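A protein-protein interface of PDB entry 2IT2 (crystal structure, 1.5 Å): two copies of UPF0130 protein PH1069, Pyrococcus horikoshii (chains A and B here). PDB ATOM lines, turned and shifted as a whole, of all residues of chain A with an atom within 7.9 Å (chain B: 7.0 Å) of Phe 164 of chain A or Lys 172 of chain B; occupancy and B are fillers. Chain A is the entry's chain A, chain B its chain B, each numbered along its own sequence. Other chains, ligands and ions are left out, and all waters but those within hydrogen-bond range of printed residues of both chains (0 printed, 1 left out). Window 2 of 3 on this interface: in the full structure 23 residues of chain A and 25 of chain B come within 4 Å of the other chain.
Of the printed residues of chain B, Gln 98 of chain A touches Ile 176 (3.3 Å). Printed residues of chain B within 4 Å of Leu 156 of chain A: Tyr 169 and Ile 176. Leu 157 of chain A touches none of the printed residues of chain B. Of chain B, only Tyr 169 (3.5 Å) and Lys 172 (3.9 Å) come within 4 Å of Phe 164 of chain A. Asn 171 of chain B touches none of the printed residues of chain A. Of chain A, only Phe 164 comes within 4 Å of Lys 172 of chain B. Of the printed residues of chain A, Ile 176 of chain B touches Gln 98 (3.3 Å) and Leu 156 (3.9 Å). The nearest residue of chain A that does not touch Lys 172 of chain B is Leu 156 of chain A (4.5 Å). The nearest printed residue of chain B that does not touch Gln 98 of chain A is Asp 179 of chain B (5.7 Å).
Tyr 169 of chain A touches its own counterpart, Tyr 169 of chain B. Position printed for both chains: 169. Of the 7 pairs that touch across the chains among the printed residues, 1 has its exchanged pair printed and touching as well.
Of the 17 printed residues of chain A, 5 touch a printed residue of chain B. Of the 15 printed residues of chain B, 3 touch a printed residue of chain A. Hydrophobic or aromatic side chains of chain B that line the printed part of chain A: Tyr 169 and Ile 176. Along chain B the printed residues that touch a printed residue of chain A span positions 169 to 176.
O of Leu 157 of chain A is in hydrogen-bond range of N of Phe 164 of chain A. The side-chain amino group of Lys 172 of chain B lies within salt-bridge range of the side-chain carboxylate of Glu 168 of chain B, at 3.98 Å.
The backbone carbonyl oxygen of Leu 156 of chain A sits at hydrogen-bond distance from the side-chain hydroxyl of Tyr 169 of chain B (2.7 Å).
Among the printed residues, merely in contact across the chains: Gln 98 of chain A with Ile 176 of chain B (3.3 Å), Phe 164 of chain A with Tyr 169 of chain B (3.5 Å), Val 165 of chain A with Tyr 169 of chain B (3.7 Å), Tyr 169 of chain A with Tyr 169 of chain B (3.8 Å), Leu 156 of chain A with Ile 176 of chain B (3.9 Å) and Phe 164 of chain A with Lys 172 of chain B (3.9 Å).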
ATOM      1  N   ILE A  91     -15.811  28.138 -27.017  1.00  0.00           N
ATOM      2  CA  ILE A  91     -14.362  28.068 -27.148  1.00  0.00           C
ATOM      3  C   ILE A  91     -13.707  29.449 -27.066  1.00  0.00           C
ATOM      4  O   ILE A  91     -12.611  29.599 -26.515  1.00  0.00           O
ATOM      5  CB  ILE A  91     -13.981  27.388 -28.472  1.00  0.00           C
ATOM      6  CG1 ILE A  91     -14.387  25.912 -28.432  1.00  0.00           C
ATOM      7  CG2 ILE A  91     -12.491  27.515 -28.719  1.00  0.00           C
ATOM      8  CD1 ILE A  91     -14.215  25.195 -29.762  1.00  0.00           C
ATOM      9  N   HIS A  94     -12.318  30.677 -23.761  1.00  0.00           N
ATOM     10  CA  HIS A  94     -11.120  30.056 -23.186  1.00  0.00           C
ATOM     11  C   HIS A  94     -10.026  31.091 -22.917  1.00  0.00           C
ATOM     12  O   HIS A  94      -9.666  31.887 -23.774  1.00  0.00           O
ATOM     13  CB  HIS A  94     -10.615  28.998 -24.180  1.00  0.00           C
ATOM     14  CG  HIS A  94      -9.296  28.412 -23.724  1.00  0.00           C
ATOM     15  ND1 HIS A  94      -9.091  27.898 -22.485  1.00  0.00           N
ATOM     16  CD2 HIS A  94      -8.127  28.235 -24.471  1.00  0.00           C
ATOM     17  CE1 HIS A  94      -7.826  27.431 -22.488  1.00  0.00           C
ATOM     18  NE2 HIS A  94      -7.224  27.619 -23.664  1.00  0.00           N
ATOM     19  N   GLY A  97      -5.330  27.426 -18.923  1.00  0.00           N
ATOM     20  CA  GLY A  97      -5.353  25.989 -18.723  1.00  0.00           C
ATOM     21  C   GLY A  97      -5.526  25.208 -20.005  1.00  0.00           C
ATOM     22  O   GLY A  97      -5.341  25.747 -21.098  1.00  0.00           O
ATOM     23  N   GLN A  98      -5.857  23.929 -19.860  1.00  0.00           N
ATOM     24  CA  GLN A  98      -6.086  23.046 -21.000  1.00  0.00           C
ATOM     25  C   GLN A  98      -7.554  23.172 -21.400  1.00  0.00           C
ATOM     26  O   GLN A  98      -8.439  23.095 -20.550  1.00  0.00           O
ATOM     27  CB  GLN A  98      -5.830  21.590 -20.616  1.00  0.00           C
ATOM     28  CG  GLN A  98      -4.547  21.334 -19.858  1.00  0.00           C
ATOM     29  CD  GLN A  98      -4.337  19.861 -19.584  1.00  0.00           C
ATOM     30  OE1 GLN A  98      -5.291  19.081 -19.536  1.00  0.00           O
ATOM     31  NE2 GLN A  98      -3.082  19.473 -19.383  1.00  0.00           N
ATOM     32  N   LEU A  99      -7.803  23.366 -22.692  1.00  0.00           N
ATOM     33  CA  LEU A  99      -9.157  23.476 -23.213  1.00  0.00           C
ATOM     34  C   LEU A  99      -9.536  22.139 -23.832  1.00  0.00           C
ATOM     35  O   LEU A  99      -8.862  21.662 -24.747  1.00  0.00           O
ATOM     36  CB  LEU A  99      -9.230  24.561 -24.279  1.00  0.00           C
ATOM     37  CG  LEU A  99     -10.593  24.726 -24.944  1.00  0.00           C
ATOM     38  CD1 LEU A  99     -11.596  25.241 -23.924  1.00  0.00           C
ATOM     39  CD2 LEU A  99     -10.483  25.700 -26.101  1.00  0.00           C
ATOM     40  N   LEU A 156      -8.549  17.340 -26.906  1.00  0.00           N
ATOM     41  CA  LEU A 156      -7.782  18.520 -26.534  1.00  0.00           C
ATOM     42  C   LEU A 156      -7.866  19.528 -27.662  1.00  0.00           C
ATOM     43  O   LEU A 156      -7.485  19.214 -28.783  1.00  0.00           O
ATOM     44  CB  LEU A 156      -6.336  18.128 -26.265  1.00  0.00           C
ATOM     45  CG  LEU A 156      -5.418  19.289 -25.907  1.00  0.00           C
ATOM     46  CD1 LEU A 156      -5.699  19.763 -24.492  1.00  0.00           C
ATOM     47  CD2 LEU A 156      -3.986  18.834 -26.035  1.00  0.00           C
ATOM     48  N   LEU A 157      -8.349  20.733 -27.368  1.00  0.00           N
ATOM     49  CA  LEU A 157      -8.544  21.785 -28.368  1.00  0.00           C
ATOM     50  C   LEU A 157      -7.536  22.940 -28.295  1.00  0.00           C
ATOM     51  O   LEU A 157      -7.325  23.671 -29.277  1.00  0.00           O
ATOM     52  CB  LEU A 157      -9.976  22.343 -28.242  1.00  0.00           C
ATOM     53  CG  LEU A 157     -11.181  21.400 -28.383  1.00  0.00           C
ATOM     54  CD1 LEU A 157     -12.497  22.180 -28.368  1.00  0.00           C
ATOM     55  CD2 LEU A 157     -11.041  20.637 -29.672  1.00  0.00           C
ATOM     56  N   GLY A 158      -6.914  23.106 -27.138  1.00  0.00           N
ATOM     57  CA  GLY A 158      -5.962  24.183 -26.982  1.00  0.00           C
ATOM     58  C   GLY A 158      -5.444  24.300 -25.567  1.00  0.00           C
ATOM     59  O   GLY A 158      -5.751  23.472 -24.714  1.00  0.00           O
ATOM     60  N   GLU A 159      -4.637  25.328 -25.323  1.00  0.00           N
ATOM     61  CA  GLU A 159      -4.087  25.537 -23.995  1.00  0.00           C
ATOM     62  C   GLU A 159      -3.695  26.986 -23.777  1.00  0.00           C
ATOM     63  O   GLU A 159      -3.229  27.664 -24.694  1.00  0.00           O
ATOM     64  CB  GLU A 159      -2.864  24.635 -23.769  1.00  0.00           C
ATOM     65  CG  GLU A 159      -2.094  24.898 -22.481  1.00  0.00           C
ATOM     66  CD  GLU A 159      -0.898  23.977 -22.308  1.00  0.00           C
ATOM     67  OE1 GLU A 159      -0.499  23.307 -23.288  1.00  0.00           O
ATOM     68  OE2 GLU A 159      -0.353  23.926 -21.185  1.00  0.00           O
ATOM     69  N   ASN A 160      -3.904  27.450 -22.554  1.00  0.00           N
ATOM     70  CA  ASN A 160      -3.570  28.806 -22.147  1.00  0.00           C
ATOM     71  C   ASN A 160      -4.002  29.903 -23.111  1.00  0.00           C
ATOM     72  O   ASN A 160      -3.208  30.774 -23.468  1.00  0.00           O
ATOM     73  CB  ASN A 160      -2.069  28.895 -21.886  1.00  0.00           C
ATOM     74  CG  ASN A 160      -1.634  28.017 -20.728  1.00  0.00           C
ATOM     75  OD1 ASN A 160      -2.107  28.181 -19.601  1.00  0.00           O
ATOM     76  ND2 ASN A 160      -0.736  27.077 -21.000  1.00  0.00           N
ATOM     77  N   GLY A 161      -5.265  29.860 -23.526  1.00  0.00           N
ATOM     78  CA  GLY A 161      -5.787  30.877 -24.422  1.00  0.00           C
ATOM     79  C   GLY A 161      -5.560  30.646 -25.903  1.00  0.00           C
ATOM     80  O   GLY A 161      -6.150  31.336 -26.735  1.00  0.00           O
ATOM     81  N   GLU A 162      -4.706  29.687 -26.242  1.00  0.00           N
ATOM     82  CA  GLU A 162      -4.433  29.395 -27.642  1.00  0.00           C
ATOM     83  C   GLU A 162      -5.203  28.182 -28.143  1.00  0.00           C
ATOM     84  O   GLU A 162      -5.065  27.084 -27.599  1.00  0.00           O
ATOM     85  CB  GLU A 162      -2.940  29.154 -27.855  1.00  0.00           C
ATOM     86  CG  GLU A 162      -2.576  28.865 -29.300  1.00  0.00           C
ATOM     87  CD  GLU A 162      -3.006  29.982 -30.240  1.00  0.00           C
ATOM     88  OE1 GLU A 162      -2.619  31.144 -29.997  1.00  0.00           O
ATOM     89  OE2 GLU A 162      -3.729  29.703 -31.223  1.00  0.00           O
ATOM     90  N   ILE A 163      -6.003  28.385 -29.185  1.00  0.00           N
ATOM     91  CA  ILE A 163      -6.785  27.306 -29.783  1.00  0.00           C
ATOM     92  C   ILE A 163      -5.912  26.641 -30.856  1.00  0.00           C
ATOM     93  O   ILE A 163      -5.319  27.329 -31.692  1.00  0.00           O
ATOM     94  CB  ILE A 163      -8.083  27.861 -30.432  1.00  0.00           C
ATOM     95  CG1 ILE A 163      -8.836  28.739 -29.422  1.00  0.00           C
ATOM     96  CG2 ILE A 163      -8.963  26.714 -30.928  1.00  0.00           C
ATOM     97  CD1 ILE A 163      -9.172  28.050 -28.102  1.00  0.00           C
ATOM     98  N   PHE A 164      -5.822  25.313 -30.840  1.00  0.00           N
ATOM     99  CA  PHE A 164      -4.987  24.615 -31.820  1.00  0.00           C
ATOM    100  C   PHE A 164      -5.708  24.175 -33.095  1.00  0.00           C
ATOM    101  O   PHE A 164      -5.065  23.901 -34.120  1.00  0.00           O
ATOM    102  CB  PHE A 164      -4.345  23.369 -31.190  1.00  0.00           C
ATOM    103  CG  PHE A 164      -3.600  23.637 -29.912  1.00  0.00           C
ATOM    104  CD1 PHE A 164      -2.832  24.786 -29.762  1.00  0.00           C
ATOM    105  CD2 PHE A 164      -3.630  22.712 -28.870  1.00  0.00           C
ATOM    106  CE1 PHE A 164      -2.109  25.017 -28.589  1.00  0.00           C
ATOM    107  CE2 PHE A 164      -2.907  22.939 -27.691  1.00  0.00           C
ATOM    108  CZ  PHE A 164      -2.146  24.089 -27.555  1.00  0.00           C
ATOM    109  N   VAL A 165      -7.033  24.102 -33.034  1.00  0.00           N
ATOM    110  CA  VAL A 165      -7.838  23.640 -34.162  1.00  0.00           C
ATOM    111  C   VAL A 165      -8.633  24.730 -34.885  1.00  0.00           C
ATOM    112  O   VAL A 165      -8.861  25.818 -34.348  1.00  0.00           O
ATOM    113  CB  VAL A 165      -8.820  22.505 -33.703  1.00  0.00           C
ATOM    114  CG1 VAL A 165      -8.056  21.412 -32.955  1.00  0.00           C
ATOM    115  CG2 VAL A 165      -9.905  23.075 -32.806  1.00  0.00           C
ATOM    116  N   GLY A 166      -9.034  24.429 -36.120  1.00  0.00           N
ATOM    117  CA  GLY A 166      -9.809  25.366 -36.924  1.00  0.00           C
ATOM    118  C   GLY A 166     -11.277  24.961 -36.978  1.00  0.00           C
ATOM    119  O   GLY A 166     -11.629  23.893 -36.475  1.00  0.00           O
ATOM    120  N   TYR A 169     -12.216  21.549 -38.575  1.00  0.00           N
ATOM    121  CA  TYR A 169     -11.895  20.463 -37.658  1.00  0.00           C
ATOM    122  C   TYR A 169     -12.992  20.354 -36.604  1.00  0.00           C
ATOM    123  O   TYR A 169     -13.477  19.259 -36.341  1.00  0.00           O
ATOM    124  CB  TYR A 169     -10.565  20.708 -36.953  1.00  0.00           C
ATOM    125  CG  TYR A 169     -10.138  19.571 -36.042  1.00  0.00           C
ATOM    126  CD1 TYR A 169      -9.392  18.508 -36.542  1.00  0.00           C
ATOM    127  CD2 TYR A 169     -10.453  19.576 -34.676  1.00  0.00           C
ATOM    128  CE1 TYR A 169      -8.952  17.488 -35.715  1.00  0.00           C
ATOM    129  CE2 TYR A 169     -10.016  18.544 -33.833  1.00  0.00           C
ATOM    130  CZ  TYR A 169      -9.257  17.508 -34.367  1.00  0.00           C
ATOM    131  OH  TYR A 169      -8.727  16.512 -33.587  1.00  0.00           O
ATOM    132  N   LEU B  84       7.923  12.064 -30.824  1.00  0.00           N
ATOM    133  CA  LEU B  84       7.209  12.548 -32.016  1.00  0.00           C
ATOM    134  C   LEU B  84       7.559  11.654 -33.202  1.00  0.00           C
ATOM    135  O   LEU B  84       6.712  11.406 -34.017  1.00  0.00           O
ATOM    136  CB  LEU B  84       7.593  13.978 -32.356  1.00  0.00           C
ATOM    137  CG  LEU B  84       6.747  14.946 -33.178  1.00  0.00           C
ATOM    138  CD1 LEU B  84       5.242  14.678 -32.985  1.00  0.00           C
ATOM    139  CD2 LEU B  84       7.192  16.375 -32.756  1.00  0.00           C
ATOM    140  N   MET B 153      -7.599  10.443 -23.661  1.00  0.00           N
ATOM    141  CA  MET B 153      -7.591  11.423 -24.738  1.00  0.00           C
ATOM    142  C   MET B 153      -8.032  10.734 -26.018  1.00  0.00           C
ATOM    143  O   MET B 153      -7.770   9.542 -26.232  1.00  0.00           O
ATOM    144  CB  MET B 153      -6.197  12.040 -24.925  1.00  0.00           C
ATOM    145  CG  MET B 153      -6.146  13.133 -26.006  1.00  0.00           C
ATOM    146  SD  MET B 153      -4.690  14.414 -25.785  1.00  0.00           S
ATOM    147  CE  MET B 153      -3.426  13.202 -25.034  1.00  0.00           C
ATOM    148  N   GLU B 167       2.838  19.706 -37.208  1.00  0.00           N
ATOM    149  CA  GLU B 167       3.793  19.336 -36.178  1.00  0.00           C
ATOM    150  C   GLU B 167       3.629  20.011 -34.833  1.00  0.00           C
ATOM    151  O   GLU B 167       3.916  19.399 -33.811  1.00  0.00           O
ATOM    152  CB  GLU B 167       5.212  19.557 -36.674  1.00  0.00           C
ATOM    153  CG  GLU B 167       6.277  18.994 -35.752  1.00  0.00           C
ATOM    154  CD  GLU B 167       7.637  18.972 -36.417  1.00  0.00           C
ATOM    155  OE1 GLU B 167       8.123  20.050 -36.817  1.00  0.00           O
ATOM    156  OE2 GLU B 167       8.218  17.873 -36.548  1.00  0.00           O
ATOM    157  N   GLU B 168       3.190  21.262 -34.820  1.00  0.00           N
ATOM    158  CA  GLU B 168       3.017  21.941 -33.547  1.00  0.00           C
ATOM    159  C   GLU B 168       1.895  21.311 -32.727  1.00  0.00           C
ATOM    160  O   GLU B 168       2.083  21.023 -31.544  1.00  0.00           O
ATOM    161  CB  GLU B 168       2.730  23.429 -33.743  1.00  0.00           C
ATOM    162  CG  GLU B 168       2.637  24.180 -32.433  1.00  0.00           C
ATOM    163  CD  GLU B 168       3.857  23.952 -31.560  1.00  0.00           C
ATOM    164  OE1 GLU B 168       4.971  24.314 -31.995  1.00  0.00           O
ATOM    165  OE2 GLU B 168       3.704  23.407 -30.445  1.00  0.00           O
ATOM    166  N   TYR B 169       0.728  21.106 -33.338  1.00  0.00           N
ATOM    167  CA  TYR B 169      -0.400  20.500 -32.634  1.00  0.00           C
ATOM    168  C   TYR B 169      -0.010  19.085 -32.237  1.00  0.00           C
ATOM    169  O   TYR B 169      -0.265  18.679 -31.107  1.00  0.00           O
ATOM    170  CB  TYR B 169      -1.662  20.515 -33.514  1.00  0.00           C
ATOM    171  CG  TYR B 169      -2.949  19.971 -32.879  1.00  0.00           C
ATOM    172  CD1 TYR B 169      -3.220  20.111 -31.514  1.00  0.00           C
ATOM    173  CD2 TYR B 169      -3.914  19.345 -33.665  1.00  0.00           C
ATOM    174  CE1 TYR B 169      -4.434  19.635 -30.952  1.00  0.00           C
ATOM    175  CE2 TYR B 169      -5.118  18.869 -33.120  1.00  0.00           C
ATOM    176  CZ  TYR B 169      -5.373  19.014 -31.764  1.00  0.00           C
ATOM    177  OH  TYR B 169      -6.560  18.515 -31.245  1.00  0.00           O
ATOM    178  N   LEU B 170       0.631  18.339 -33.133  1.00  0.00           N
ATOM    179  CA  LEU B 170       1.032  16.975 -32.796  1.00  0.00           C
ATOM    180  C   LEU B 170       1.998  16.983 -31.603  1.00  0.00           C
ATOM    181  O   LEU B 170       1.923  16.108 -30.737  1.00  0.00           O
ATOM    182  CB  LEU B 170       1.670  16.273 -34.002  1.00  0.00           C
ATOM    183  CG  LEU B 170       1.935  14.773 -33.788  1.00  0.00           C
ATOM    184  CD1 LEU B 170       0.617  14.053 -33.527  1.00  0.00           C
ATOM    185  CD2 LEU B 170       2.615  14.186 -35.004  1.00  0.00           C
ATOM    186  N   ASN B 171       2.882  17.977 -31.537  1.00  0.00           N
ATOM    187  CA  ASN B 171       3.818  18.077 -30.417  1.00  0.00           C
ATOM    188  C   ASN B 171       3.089  18.308 -29.089  1.00  0.00           C
ATOM    189  O   ASN B 171       3.464  17.732 -28.065  1.00  0.00           O
ATOM    190  CB  ASN B 171       4.813  19.208 -30.640  1.00  0.00           C
ATOM    191  CG  ASN B 171       5.767  19.362 -29.484  1.00  0.00           C
ATOM    192  OD1 ASN B 171       5.849  20.429 -28.874  1.00  0.00           O
ATOM    193  ND2 ASN B 171       6.501  18.301 -29.176  1.00  0.00           N
ATOM    194  N   LYS B 172       2.059  19.149 -29.106  1.00  0.00           N
ATOM    195  CA  LYS B 172       1.277  19.415 -27.898  1.00  0.00           C
ATOM    196  C   LYS B 172       0.501  18.159 -27.480  1.00  0.00           C
ATOM    197  O   LYS B 172       0.416  17.854 -26.293  1.00  0.00           O
ATOM    198  CB  LYS B 172       0.298  20.575 -28.125  1.00  0.00           C
ATOM    199  CG  LYS B 172       0.948  21.910 -28.459  1.00  0.00           C
ATOM    200  CD  LYS B 172       1.823  22.400 -27.321  1.00  0.00           C
ATOM    201  CE  LYS B 172       2.442  23.743 -27.646  1.00  0.00           C
ATOM    202  NZ  LYS B 172       3.351  24.184 -26.556  1.00  0.00           N
ATOM    203  N   ILE B 173      -0.058  17.424 -28.441  1.00  0.00           N
ATOM    204  CA  ILE B 173      -0.807  16.205 -28.134  1.00  0.00           C
ATOM    205  C   ILE B 173       0.112  15.154 -27.506  1.00  0.00           C
ATOM    206  O   ILE B 173      -0.264  14.490 -26.528  1.00  0.00           O
ATOM    207  CB  ILE B 173      -1.446  15.621 -29.418  1.00  0.00           C
ATOM    208  CG1 ILE B 173      -2.520  16.579 -29.930  1.00  0.00           C
ATOM    209  CG2 ILE B 173      -2.002  14.221 -29.160  1.00  0.00           C
ATOM    210  CD1 ILE B 173      -3.004  16.263 -31.338  1.00  0.00           C
ATOM    211  N   VAL B 174       1.307  14.992 -28.068  1.00  0.00           N
ATOM    212  CA  VAL B 174       2.257  14.018 -27.533  1.00  0.00           C
ATOM    213  C   VAL B 174       2.701  14.393 -26.120  1.00  0.00           C
ATOM    214  O   VAL B 174       2.879  13.516 -25.271  1.00  0.00           O
ATOM    215  CB  VAL B 174       3.493  13.887 -28.451  1.00  0.00           C
ATOM    216  CG1 VAL B 174       4.635  13.165 -27.732  1.00  0.00           C
ATOM    217  CG2 VAL B 174       3.117  13.116 -29.693  1.00  0.00           C
ATOM    218  N   GLU B 175       2.866  15.689 -25.866  1.00  0.00           N
ATOM    219  CA  GLU B 175       3.265  16.179 -24.550  1.00  0.00           C
ATOM    220  C   GLU B 175       2.224  15.786 -23.503  1.00  0.00           C
ATOM    221  O   GLU B 175       2.563  15.225 -22.461  1.00  0.00           O
ATOM    222  CB  GLU B 175       3.389  17.699 -24.590  1.00  0.00           C
ATOM    223  CG  GLU B 175       3.928  18.363 -23.349  1.00  0.00           C
ATOM    224  CD  GLU B 175       3.805  19.874 -23.445  1.00  0.00           C
ATOM    225  OE1 GLU B 175       4.001  20.420 -24.555  1.00  0.00           O
ATOM    226  OE2 GLU B 175       3.514  20.519 -22.415  1.00  0.00           O
ATOM    227  N   ILE B 176       0.960  16.091 -23.774  1.00  0.00           N
ATOM    228  CA  ILE B 176      -0.113  15.758 -22.840  1.00  0.00           C
ATOM    229  C   ILE B 176      -0.222  14.245 -22.697  1.00  0.00           C
ATOM    230  O   ILE B 176      -0.385  13.729 -21.594  1.00  0.00           O
ATOM    231  CB  ILE B 176      -1.461  16.344 -23.327  1.00  0.00           C
ATOM    232  CG1 ILE B 176      -1.368  17.873 -23.344  1.00  0.00           C
ATOM    233  CG2 ILE B 176      -2.611  15.874 -22.428  1.00  0.00           C
ATOM    234  CD1 ILE B 176      -1.237  18.501 -21.967  1.00  0.00           C
ATOM    235  N   ALA B 177      -0.126  13.530 -23.813  1.00  0.00           N
ATOM    236  CA  ALA B 177      -0.225  12.077 -23.778  1.00  0.00           C
ATOM    237  C   ALA B 177       0.831  11.491 -22.867  1.00  0.00           C
ATOM    238  O   ALA B 177       0.541  10.589 -22.084  1.00  0.00           O
ATOM    239  CB  ALA B 177      -0.071  11.500 -25.170  1.00  0.00           C
ATOM    240  N   ASN B 178       2.057  11.994 -22.979  1.00  0.00           N
ATOM    241  CA  ASN B 178       3.149  11.502 -22.148  1.00  0.00           C
ATOM    242  C   ASN B 178       2.937  11.881 -20.685  1.00  0.00           C
ATOM    243  O   ASN B 178       3.369  11.147 -19.804  1.00  0.00           O
ATOM    244  CB  ASN B 178       4.508  12.021 -22.647  1.00  0.00           C
ATOM    245  CG  ASN B 178       4.970  11.315 -23.921  1.00  0.00           C
ATOM    246  OD1 ASN B 178       4.574  10.181 -24.199  1.00  0.00           O
ATOM    247  ND2 ASN B 178       5.829  11.980 -24.688  1.00  0.00           N
ATOM    248  N   ASP B 179       2.285  13.015 -20.428  1.00  0.00           N
ATOM    249  CA  ASP B 179       1.999  13.426 -19.053  1.00  0.00           C
ATOM    250  C   ASP B 179       0.997  12.457 -18.454  1.00  0.00           C
ATOM    251  O   ASP B 179       1.129  12.053 -17.304  1.00  0.00           O
ATOM    252  CB  ASP B 179       1.404  14.831 -19.008  1.00  0.00           C
ATOM    253  CG  ASP B 179       2.405  15.891 -19.360  1.00  0.00           C
ATOM    254  OD1 ASP B 179       3.616  15.641 -19.184  1.00  0.00           O
ATOM    255  OD2 ASP B 179       1.982  16.977 -19.800  1.00  0.00           O
